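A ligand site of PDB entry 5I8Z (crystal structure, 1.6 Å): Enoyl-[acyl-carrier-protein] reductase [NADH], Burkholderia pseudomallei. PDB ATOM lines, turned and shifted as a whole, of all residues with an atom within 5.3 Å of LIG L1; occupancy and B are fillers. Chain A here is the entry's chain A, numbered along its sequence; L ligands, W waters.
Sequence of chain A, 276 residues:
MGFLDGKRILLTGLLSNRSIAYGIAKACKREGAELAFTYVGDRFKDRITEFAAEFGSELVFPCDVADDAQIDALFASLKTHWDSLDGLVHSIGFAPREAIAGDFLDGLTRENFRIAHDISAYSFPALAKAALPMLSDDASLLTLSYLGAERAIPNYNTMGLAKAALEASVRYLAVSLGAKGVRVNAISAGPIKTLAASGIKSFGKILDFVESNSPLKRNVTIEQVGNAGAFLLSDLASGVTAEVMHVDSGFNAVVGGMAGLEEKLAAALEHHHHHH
The side-chain hydroxyl (OH) of Tyr 156 is in hydrogen-bond range of an oxygen (O1) of LIG L1, at 2.5 Å. The backbone NH (N) of Ala 95 is in hydrogen-bond range of an oxygen (O4) of LIG L1 (3.2 Å). O1 of LG2 L2 lies within hydrogen-bond range of N of Ala 196. An oxygen (O13) of LG2 L2 lies within hydrogen-bond range of the side-chain amino group (NZ) of Lys 163 (2.8 Å). The side-chain hydroxyl of Thr 194 sits at hydrogen-bond distance from an oxygen (O8) of LG2 L2. The backbone NH of Ile 192 sits at hydrogen-bond distance from an oxygen (O14) of LG2 L2, 2.8 Å away. O of Ile 192 is in hydrogen-bond range of N7 of LG2 L2.
O13 of LG2 L2 sits at hydrogen-bond distance from O1 of LIG L1.
N of Ala 196 sits close to OG1 of Thr 194, 3.3 Å away.
Gly 93 touches LIG L1 (O to C5, 3.4 Å). CA of Phe 94 touches O4 of LIG L1, 3.4 Å away. CD1 of Ile 100 touches O3 of LIG L1, 3.5 Å away. Tyr 146 touches LIG L1 (CE1 to C12, 3.8 Å). Pro 154 touches LIG L1 (O to C16, 3.7 Å). C of Asn 155 touches C17 of LIG L1 (3.8 Å). Met 159 touches LIG L1 (CE to C6, 3.7 Å). Lys 163 touches LIG L1 (CE to O1, 3.8 Å). Ala 196 touches LIG L1 (CB to C4, 3.5 Å). Ile 200 touches LIG L1 (CG2 to C17, 3.7 Å). Phe 203 touches LIG L1 (CE1 to C13, 3.9 Å). Hydrophobic or aromatic side chains within 4 Å of LIG L1: Phe 94, Ala 95, Ile 100, Tyr 146, Tyr 156, Met 159, Ala 196, Ile 200 and Phe 203. Of the 21 residues printed, 13 come within 4 Å of LIG L1.
Water W1 lies within hydrogen-bond range of the backbone carbonyl oxygen (O) of Ala 95 (2.7 Å) and an oxygen (O4) of LIG L1 (3.1 Å).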
ATOM      1  N   GLY A  93     -27.938 -27.006  -2.166  1.00  0.00           N
ATOM      2  CA  GLY A  93     -27.471 -26.883  -0.771  1.00  0.00           C
ATOM      3  C   GLY A  93     -27.517 -25.398  -0.422  1.00  0.00           C
ATOM      4  O   GLY A  93     -27.326 -24.538  -1.305  1.00  0.00           O
ATOM      5  N   PHE A  94     -27.791 -25.098   0.847  1.00  0.00           N
ATOM      6  CA  PHE A  94     -27.742 -23.714   1.316  1.00  0.00           C
ATOM      7  C   PHE A  94     -27.678 -23.715   2.849  1.00  0.00           C
ATOM      8  O   PHE A  94     -28.432 -24.470   3.505  1.00  0.00           O
ATOM      9  CB  PHE A  94     -28.991 -22.938   0.883  1.00  0.00           C
ATOM     10  CG  PHE A  94     -29.020 -21.551   1.412  1.00  0.00           C
ATOM     11  CD1 PHE A  94     -28.242 -20.549   0.813  1.00  0.00           C
ATOM     12  CD2 PHE A  94     -29.799 -21.217   2.498  1.00  0.00           C
ATOM     13  CE1 PHE A  94     -28.231 -19.271   1.297  1.00  0.00           C
ATOM     14  CE2 PHE A  94     -29.791 -19.903   3.003  1.00  0.00           C
ATOM     15  CZ  PHE A  94     -29.014 -18.958   2.414  1.00  0.00           C
ATOM     16  N   ALA A  95     -26.829 -22.832   3.390  1.00  0.00           N
ATOM     17  CA  ALA A  95     -26.890 -22.404   4.794  1.00  0.00           C
ATOM     18  C   ALA A  95     -26.596 -20.930   4.822  1.00  0.00           C
ATOM     19  O   ALA A  95     -25.817 -20.439   4.044  1.00  0.00           O
ATOM     20  CB  ALA A  95     -25.845 -23.153   5.663  1.00  0.00           C
ATOM     21  N   PRO A  96     -27.180 -20.230   5.792  1.00  0.00           N
ATOM     22  CA  PRO A  96     -26.739 -18.838   5.944  1.00  0.00           C
ATOM     23  C   PRO A  96     -25.228 -18.700   6.150  1.00  0.00           C
ATOM     24  O   PRO A  96     -24.585 -19.549   6.785  1.00  0.00           O
ATOM     25  CB  PRO A  96     -27.523 -18.375   7.190  1.00  0.00           C
ATOM     26  CG  PRO A  96     -28.792 -19.263   7.202  1.00  0.00           C
ATOM     27  CD  PRO A  96     -28.225 -20.615   6.751  1.00  0.00           C
ATOM     28  N   ILE A 100     -21.434 -21.199   8.330  1.00  0.00           N
ATOM     29  CA  ILE A 100     -20.367 -21.993   7.687  1.00  0.00           C
ATOM     30  C   ILE A 100     -19.079 -21.233   7.634  1.00  0.00           C
ATOM     31  O   ILE A 100     -18.220 -21.448   6.770  1.00  0.00           O
ATOM     32  CB  ILE A 100     -20.685 -22.399   6.257  1.00  0.00           C
ATOM     33  CG1 ILE A 100     -20.809 -21.186   5.358  1.00  0.00           C
ATOM     34  CG2 ILE A 100     -21.918 -23.176   6.173  1.00  0.00           C
ATOM     35  CD1 ILE A 100     -20.426 -21.549   3.946  1.00  0.00           C
ATOM     36  N   TYR A 146     -21.146 -34.361   0.992  1.00  0.00           N
ATOM     37  CA  TYR A 146     -19.742 -34.035   1.180  1.00  0.00           C
ATOM     38  C   TYR A 146     -19.253 -34.735   2.456  1.00  0.00           C
ATOM     39  O   TYR A 146     -20.045 -34.969   3.395  1.00  0.00           O
ATOM     40  CB  TYR A 146     -19.587 -32.490   1.273  1.00  0.00           C
ATOM     41  CG  TYR A 146     -18.145 -32.081   1.506  1.00  0.00           C
ATOM     42  CD1 TYR A 146     -17.172 -32.456   0.580  1.00  0.00           C
ATOM     43  CD2 TYR A 146     -17.789 -31.411   2.669  1.00  0.00           C
ATOM     44  CE1 TYR A 146     -15.870 -32.119   0.809  1.00  0.00           C
ATOM     45  CE2 TYR A 146     -16.456 -31.046   2.915  1.00  0.00           C
ATOM     46  CZ  TYR A 146     -15.512 -31.463   1.992  1.00  0.00           C
ATOM     47  OH  TYR A 146     -14.162 -31.191   2.226  1.00  0.00           O
ATOM     48  N   ILE A 153     -15.092 -31.061   9.511  1.00  0.00           N
ATOM     49  CA  ILE A 153     -14.176 -30.288   8.645  1.00  0.00           C
ATOM     50  C   ILE A 153     -14.327 -28.848   9.027  1.00  0.00           C
ATOM     51  O   ILE A 153     -15.429 -28.354   9.233  1.00  0.00           O
ATOM     52  CB  ILE A 153     -14.537 -30.494   7.148  1.00  0.00           C
ATOM     53  CG1 ILE A 153     -14.405 -32.010   6.819  1.00  0.00           C
ATOM     54  CG2 ILE A 153     -13.619 -29.663   6.282  1.00  0.00           C
ATOM     55  CD1 ILE A 153     -14.480 -32.447   5.351  1.00  0.00           C
ATOM     56  N   PRO A 154     -13.196 -28.115   9.173  1.00  0.00           N
ATOM     57  CA  PRO A 154     -13.384 -26.764   9.691  1.00  0.00           C
ATOM     58  C   PRO A 154     -14.239 -25.917   8.769  1.00  0.00           C
ATOM     59  O   PRO A 154     -14.173 -26.088   7.554  1.00  0.00           O
ATOM     60  CB  PRO A 154     -11.953 -26.214   9.783  1.00  0.00           C
ATOM     61  CG  PRO A 154     -11.116 -27.450   9.965  1.00  0.00           C
ATOM     62  CD  PRO A 154     -11.783 -28.514   9.092  1.00  0.00           C
ATOM     63  N   ASN A 155     -15.070 -25.069   9.394  1.00  0.00           N
ATOM     64  CA  ASN A 155     -16.007 -24.152   8.783  1.00  0.00           C
ATOM     65  C   ASN A 155     -17.270 -24.799   8.209  1.00  0.00           C
ATOM     66  O   ASN A 155     -18.297 -24.155   8.143  1.00  0.00           O
ATOM     67  CB  ASN A 155     -15.313 -23.314   7.701  1.00  0.00           C
ATOM     68  CG  ASN A 155     -14.215 -22.412   8.293  1.00  0.00           C
ATOM     69  OD1 ASN A 155     -14.502 -21.375   8.874  1.00  0.00           O
ATOM     70  ND2 ASN A 155     -12.967 -22.834   8.150  1.00  0.00           N
ATOM     71  N   TYR A 156     -17.221 -26.078   7.868  1.00  0.00           N
ATOM     72  CA  TYR A 156     -18.438 -26.650   7.238  1.00  0.00           C
ATOM     73  C   TYR A 156     -19.606 -26.648   8.219  1.00  0.00           C
ATOM     74  O   TYR A 156     -20.770 -26.448   7.820  1.00  0.00           O
ATOM     75  CB  TYR A 156     -18.158 -28.069   6.730  1.00  0.00           C
ATOM     76  CG  TYR A 156     -19.080 -28.566   5.602  1.00  0.00           C
ATOM     77  CD1 TYR A 156     -19.160 -27.867   4.409  1.00  0.00           C
ATOM     78  CD2 TYR A 156     -19.792 -29.731   5.731  1.00  0.00           C
ATOM     79  CE1 TYR A 156     -19.987 -28.326   3.350  1.00  0.00           C
ATOM     80  CE2 TYR A 156     -20.609 -30.217   4.762  1.00  0.00           C
ATOM     81  CZ  TYR A 156     -20.712 -29.497   3.552  1.00  0.00           C
ATOM     82  OH  TYR A 156     -21.508 -29.956   2.509  1.00  0.00           O
ATOM     83  N   MET A 159     -23.634 -27.092   7.935  1.00  0.00           N
ATOM     84  CA  MET A 159     -23.852 -27.875   6.717  1.00  0.00           C
ATOM     85  C   MET A 159     -23.460 -29.346   6.951  1.00  0.00           C
ATOM     86  O   MET A 159     -24.021 -30.215   6.307  1.00  0.00           O
ATOM     87  CB  MET A 159     -23.038 -27.284   5.531  1.00  0.00           C
ATOM     88  CG  MET A 159     -23.370 -27.900   4.184  1.00  0.00           C
ATOM     89  SD  MET A 159     -25.117 -27.684   3.722  1.00  0.00           S
ATOM     90  CE  MET A 159     -25.071 -25.993   3.133  1.00  0.00           C
ATOM     91  N   LYS A 163     -25.811 -32.359   5.973  1.00  0.00           N
ATOM     92  CA  LYS A 163     -25.443 -33.438   5.061  1.00  0.00           C
ATOM     93  C   LYS A 163     -25.522 -34.801   5.742  1.00  0.00           C
ATOM     94  O   LYS A 163     -25.825 -35.808   5.038  1.00  0.00           O
ATOM     95  CB  LYS A 163     -24.031 -33.234   4.503  1.00  0.00           C
ATOM     96  CG  LYS A 163     -23.888 -32.032   3.573  1.00  0.00           C
ATOM     97  CD  LYS A 163     -24.806 -32.185   2.292  1.00  0.00           C
ATOM     98  CE  LYS A 163     -24.376 -31.059   1.349  1.00  0.00           C
ATOM     99  NZ  LYS A 163     -25.225 -31.080   0.059  1.00  0.00           N
ATOM    100  N   PRO A 191     -14.038 -31.488  -3.284  1.00  0.00           N
ATOM    101  CA  PRO A 191     -14.186 -30.040  -3.496  1.00  0.00           C
ATOM    102  C   PRO A 191     -14.001 -29.724  -4.969  1.00  0.00           C
ATOM    103  O   PRO A 191     -13.079 -30.187  -5.628  1.00  0.00           O
ATOM    104  CB  PRO A 191     -13.050 -29.427  -2.656  1.00  0.00           C
ATOM    105  CG  PRO A 191     -12.060 -30.620  -2.462  1.00  0.00           C
ATOM    106  CD  PRO A 191     -12.934 -31.836  -2.363  1.00  0.00           C
ATOM    107  N   ILE A 192     -14.896 -28.863  -5.444  1.00  0.00           N
ATOM    108  CA  ILE A 192     -14.926 -28.388  -6.802  1.00  0.00           C
ATOM    109  C   ILE A 192     -15.264 -26.909  -6.762  1.00  0.00           C
ATOM    110  O   ILE A 192     -16.177 -26.481  -6.064  1.00  0.00           O
ATOM    111  CB  ILE A 192     -15.956 -29.133  -7.665  1.00  0.00           C
ATOM    112  CG1 ILE A 192     -15.566 -30.609  -7.813  1.00  0.00           C
ATOM    113  CG2 ILE A 192     -16.043 -28.514  -9.068  1.00  0.00           C
ATOM    114  CD1 ILE A 192     -16.693 -31.475  -8.482  1.00  0.00           C
ATOM    115  N   THR A 194     -17.114 -24.242  -7.538  1.00  0.00           N
ATOM    116  CA  THR A 194     -18.415 -23.790  -8.044  1.00  0.00           C
ATOM    117  C   THR A 194     -18.787 -22.480  -7.434  1.00  0.00           C
ATOM    118  O   THR A 194     -18.047 -21.957  -6.597  1.00  0.00           O
ATOM    119  CB  THR A 194     -19.516 -24.774  -7.719  1.00  0.00           C
ATOM    120  OG1 THR A 194     -19.635 -24.839  -6.265  1.00  0.00           O
ATOM    121  CG2 THR A 194     -19.191 -26.174  -8.262  1.00  0.00           C
ATOM    122  N   ALA A 196     -21.110 -22.007  -5.284  1.00  0.00           N
ATOM    123  CA  ALA A 196     -21.387 -22.172  -3.862  1.00  0.00           C
ATOM    124  C   ALA A 196     -20.028 -22.213  -3.123  1.00  0.00           C
ATOM    125  O   ALA A 196     -19.908 -21.726  -2.023  1.00  0.00           O
ATOM    126  CB  ALA A 196     -22.212 -23.466  -3.617  1.00  0.00           C
ATOM    127  N   ALA A 197     -19.030 -22.814  -3.760  1.00  0.00           N
ATOM    128  CA  ALA A 197     -17.742 -22.995  -3.093  1.00  0.00           C
ATOM    129  C   ALA A 197     -17.057 -21.649  -2.969  1.00  0.00           C
ATOM    130  O   ALA A 197     -16.229 -21.441  -2.110  1.00  0.00           O
ATOM    131  CB  ALA A 197     -16.871 -23.995  -3.873  1.00  0.00           C
ATOM    132  N   ILE A 200     -16.634 -19.501   0.312  1.00  0.00           N
ATOM    133  CA  ILE A 200     -15.897 -20.108   1.428  1.00  0.00           C
ATOM    134  C   ILE A 200     -14.444 -19.665   1.438  1.00  0.00           C
ATOM    135  O   ILE A 200     -13.681 -20.060   0.546  1.00  0.00           O
ATOM    136  CB  ILE A 200     -15.976 -21.620   1.305  1.00  0.00           C
ATOM    137  CG1 ILE A 200     -17.454 -22.048   1.187  1.00  0.00           C
ATOM    138  CG2 ILE A 200     -15.173 -22.371   2.424  1.00  0.00           C
ATOM    139  CD1 ILE A 200     -17.669 -23.509   0.798  1.00  0.00           C
ATOM    140  N   SER A 202     -11.832 -20.401   3.041  1.00  0.00           N
ATOM    141  CA  SER A 202     -10.784 -21.399   3.166  1.00  0.00           C
ATOM    142  C   SER A 202     -10.769 -22.396   2.002  1.00  0.00           C
ATOM    143  O   SER A 202     -10.001 -23.354   2.039  1.00  0.00           O
ATOM    144  CB  SER A 202     -10.909 -22.187   4.464  1.00  0.00           C
ATOM    145  OG  SER A 202     -12.070 -22.974   4.452  1.00  0.00           O
ATOM    146  N   PHE A 203     -11.619 -22.187   0.993  1.00  0.00           N
ATOM    147  CA  PHE A 203     -11.758 -23.183  -0.083  1.00  0.00           C
ATOM    148  C   PHE A 203     -10.478 -23.443  -0.875  1.00  0.00           C
ATOM    149  O   PHE A 203     -10.146 -24.606  -1.138  1.00  0.00           O
ATOM    150  CB  PHE A 203     -12.900 -22.785  -1.050  1.00  0.00           C
ATOM    151  CG  PHE A 203     -13.285 -23.883  -1.995  1.00  0.00           C
ATOM    152  CD1 PHE A 203     -14.044 -24.972  -1.569  1.00  0.00           C
ATOM    153  CD2 PHE A 203     -12.837 -23.845  -3.306  1.00  0.00           C
ATOM    154  CE1 PHE A 203     -14.389 -25.994  -2.499  1.00  0.00           C
ATOM    155  CE2 PHE A 203     -13.171 -24.874  -4.208  1.00  0.00           C
ATOM    156  CZ  PHE A 203     -13.922 -25.942  -3.782  1.00  0.00           C
ATOM    157  N   ILE A 206      -8.443 -25.935   1.067  1.00  0.00           N
ATOM    158  CA  ILE A 206      -9.005 -27.307   0.969  1.00  0.00           C
ATOM    159  C   ILE A 206      -8.604 -27.946  -0.372  1.00  0.00           C
ATOM    160  O   ILE A 206      -8.192 -29.125  -0.444  1.00  0.00           O
ATOM    161  CB  ILE A 206     -10.540 -27.270   1.108  1.00  0.00           C
ATOM    162  CG1 ILE A 206     -10.945 -26.546   2.389  1.00  0.00           C
ATOM    163  CG2 ILE A 206     -11.122 -28.690   1.042  1.00  0.00           C
ATOM    164  CD1 ILE A 206     -10.312 -27.133   3.577  1.00  0.00           C
HETATM  165  C1  LIG L   1     -20.441 -28.153  -0.202  1.00  0.00           C
HETATM  166  N1  LIG L   1     -24.044 -22.421   1.634  1.00  0.00           N
HETATM  167  O1  LIG L   1     -21.589 -28.759   0.267  1.00  0.00           O
HETATM  168  C2  LIG L   1     -20.634 -27.050  -1.042  1.00  0.00           C
HETATM  169  O2  LIG L   1     -21.918 -26.581  -1.288  1.00  0.00           O
HETATM  170  C3  LIG L   1     -22.387 -25.570  -0.484  1.00  0.00           C
HETATM  171  O3  LIG L   1     -23.645 -22.171   2.774  1.00  0.00           O
HETATM  172  C4  LIG L   1     -23.651 -25.054  -0.884  1.00  0.00           C
HETATM  173  O4  LIG L   1     -24.989 -21.772   1.055  1.00  0.00           O
HETATM  174  C5  LIG L   1     -24.156 -24.014  -0.156  1.00  0.00           C
HETATM  175  C6  LIG L   1     -23.456 -23.494   0.897  1.00  0.00           C
HETATM  176  C7  LIG L   1     -22.240 -24.000   1.312  1.00  0.00           C
HETATM  177  C8  LIG L   1     -21.702 -25.063   0.571  1.00  0.00           C
HETATM  178  C9  LIG L   1     -19.487 -26.474  -1.622  1.00  0.00           C
HETATM  179  C10 LIG L   1     -18.239 -26.976  -1.361  1.00  0.00           C
HETATM  180  C11 LIG L   1     -18.098 -28.070  -0.546  1.00  0.00           C
HETATM  181  C12 LIG L   1     -16.725 -28.592  -0.310  1.00  0.00           C
HETATM  182  C13 LIG L   1     -15.879 -27.789   0.604  1.00  0.00           C
HETATM  183  C14 LIG L   1     -16.406 -27.371   1.931  1.00  0.00           C
HETATM  184  C15 LIG L   1     -15.393 -26.660   2.846  1.00  0.00           C
HETATM  185  C16 LIG L   1     -15.823 -26.281   4.213  1.00  0.00           C
HETATM  186  C17 LIG L   1     -16.658 -25.041   4.424  1.00  0.00           C
HETATM  187  C18 LIG L   1     -19.207 -28.719   0.020  1.00  0.00           C
HETATM  188  P1  LG2 L   2     -23.810 -24.428  -7.211  1.00  0.00           P
HETATM  189  O1  LG2 L   2     -23.638 -23.126  -6.574  1.00  0.00           O
HETATM  190  O2  LG2 L   2     -23.473 -24.585  -8.669  1.00  0.00           O
HETATM  191  O3  LG2 L   2     -25.228 -25.131  -7.012  1.00  0.00           O
HETATM  192  C1  LG2 L   2     -25.884 -24.907  -5.749  1.00  0.00           C
HETATM  193  C2  LG2 L   2     -27.337 -24.900  -6.174  1.00  0.00           C
HETATM  194  O4  LG2 L   2     -28.153 -24.882  -4.992  1.00  0.00           O
HETATM  195  C3  LG2 L   2     -27.727 -23.704  -7.032  1.00  0.00           C
HETATM  196  O5  LG2 L   2     -28.172 -24.137  -8.246  1.00  0.00           O
HETATM  197  C4  LG2 L   2     -28.766 -23.135  -6.189  1.00  0.00           C
HETATM  198  O6  LG2 L   2     -29.764 -22.458  -6.993  1.00  0.00           O
HETATM  199  C5  LG2 L   2     -29.341 -24.292  -5.431  1.00  0.00           C
HETATM  200  N1  LG2 L   2     -30.218 -23.848  -4.315  1.00  0.00           N
HETATM  201  C6  LG2 L   2     -29.829 -23.194  -3.226  1.00  0.00           C
HETATM  202  N2  LG2 L   2     -31.003 -22.848  -2.487  1.00  0.00           N
HETATM  203  C7  LG2 L   2     -32.047 -23.435  -3.279  1.00  0.00           C
HETATM  204  C8  LG2 L   2     -33.506 -23.343  -2.999  1.00  0.00           C
HETATM  205  N3  LG2 L   2     -34.013 -22.603  -1.867  1.00  0.00           N
HETATM  206  N4  LG2 L   2     -34.259 -23.902  -3.875  1.00  0.00           N
HETATM  207  C9  LG2 L   2     -33.774 -24.606  -5.024  1.00  0.00           C
HETATM  208  N5  LG2 L   2     -32.347 -24.605  -5.311  1.00  0.00           N
HETATM  209  C10 LG2 L   2     -31.496 -23.979  -4.347  1.00  0.00           C
HETATM  210  O7  LG2 L   2     -22.851 -25.379  -6.331  1.00  0.00           O
HETATM  211  P2  LG2 L   2     -22.562 -26.941  -6.396  1.00  0.00           P
HETATM  212  O8  LG2 L   2     -21.224 -26.969  -5.726  1.00  0.00           O
HETATM  213  O9  LG2 L   2     -22.711 -27.572  -7.694  1.00  0.00           O
HETATM  214  O10 LG2 L   2     -23.668 -27.514  -5.338  1.00  0.00           O
HETATM  215  C11 LG2 L   2     -24.414 -28.605  -5.718  1.00  0.00           C
HETATM  216  C12 LG2 L   2     -24.542 -29.550  -4.509  1.00  0.00           C
HETATM  217  O11 LG2 L   2     -23.260 -30.210  -4.393  1.00  0.00           O
HETATM  218  C13 LG2 L   2     -24.884 -28.962  -3.184  1.00  0.00           C
HETATM  219  O12 LG2 L   2     -25.681 -29.856  -2.483  1.00  0.00           O
HETATM  220  C14 LG2 L   2     -23.549 -28.982  -2.484  1.00  0.00           C
HETATM  221  O13 LG2 L   2     -23.733 -29.031  -1.103  1.00  0.00           O
HETATM  222  C15 LG2 L   2     -22.966 -30.215  -3.018  1.00  0.00           C
HETATM  223  N6  LG2 L   2     -21.493 -30.374  -2.916  1.00  0.00           N
HETATM  224  C16 LG2 L   2     -20.713 -29.359  -3.506  1.00  0.00           C
HETATM  225  C17 LG2 L   2     -19.162 -29.586  -3.504  1.00  0.00           C
HETATM  226  C18 LG2 L   2     -18.266 -28.624  -4.117  1.00  0.00           C
HETATM  227  O14 LG2 L   2     -17.070 -28.797  -3.702  1.00  0.00           O
HETATM  228  N7  LG2 L   2     -18.799 -27.798  -5.026  1.00  0.00           N
HETATM  229  C19 LG2 L   2     -18.693 -30.837  -2.867  1.00  0.00           C
HETATM  230  C20 LG2 L   2     -19.629 -31.643  -2.411  1.00  0.00           C
HETATM  231  C21 LG2 L   2     -20.864 -31.422  -2.450  1.00  0.00           C
HETATM  232  O   HOH W   1     -24.711 -18.885   2.134  1.00  0.00           O
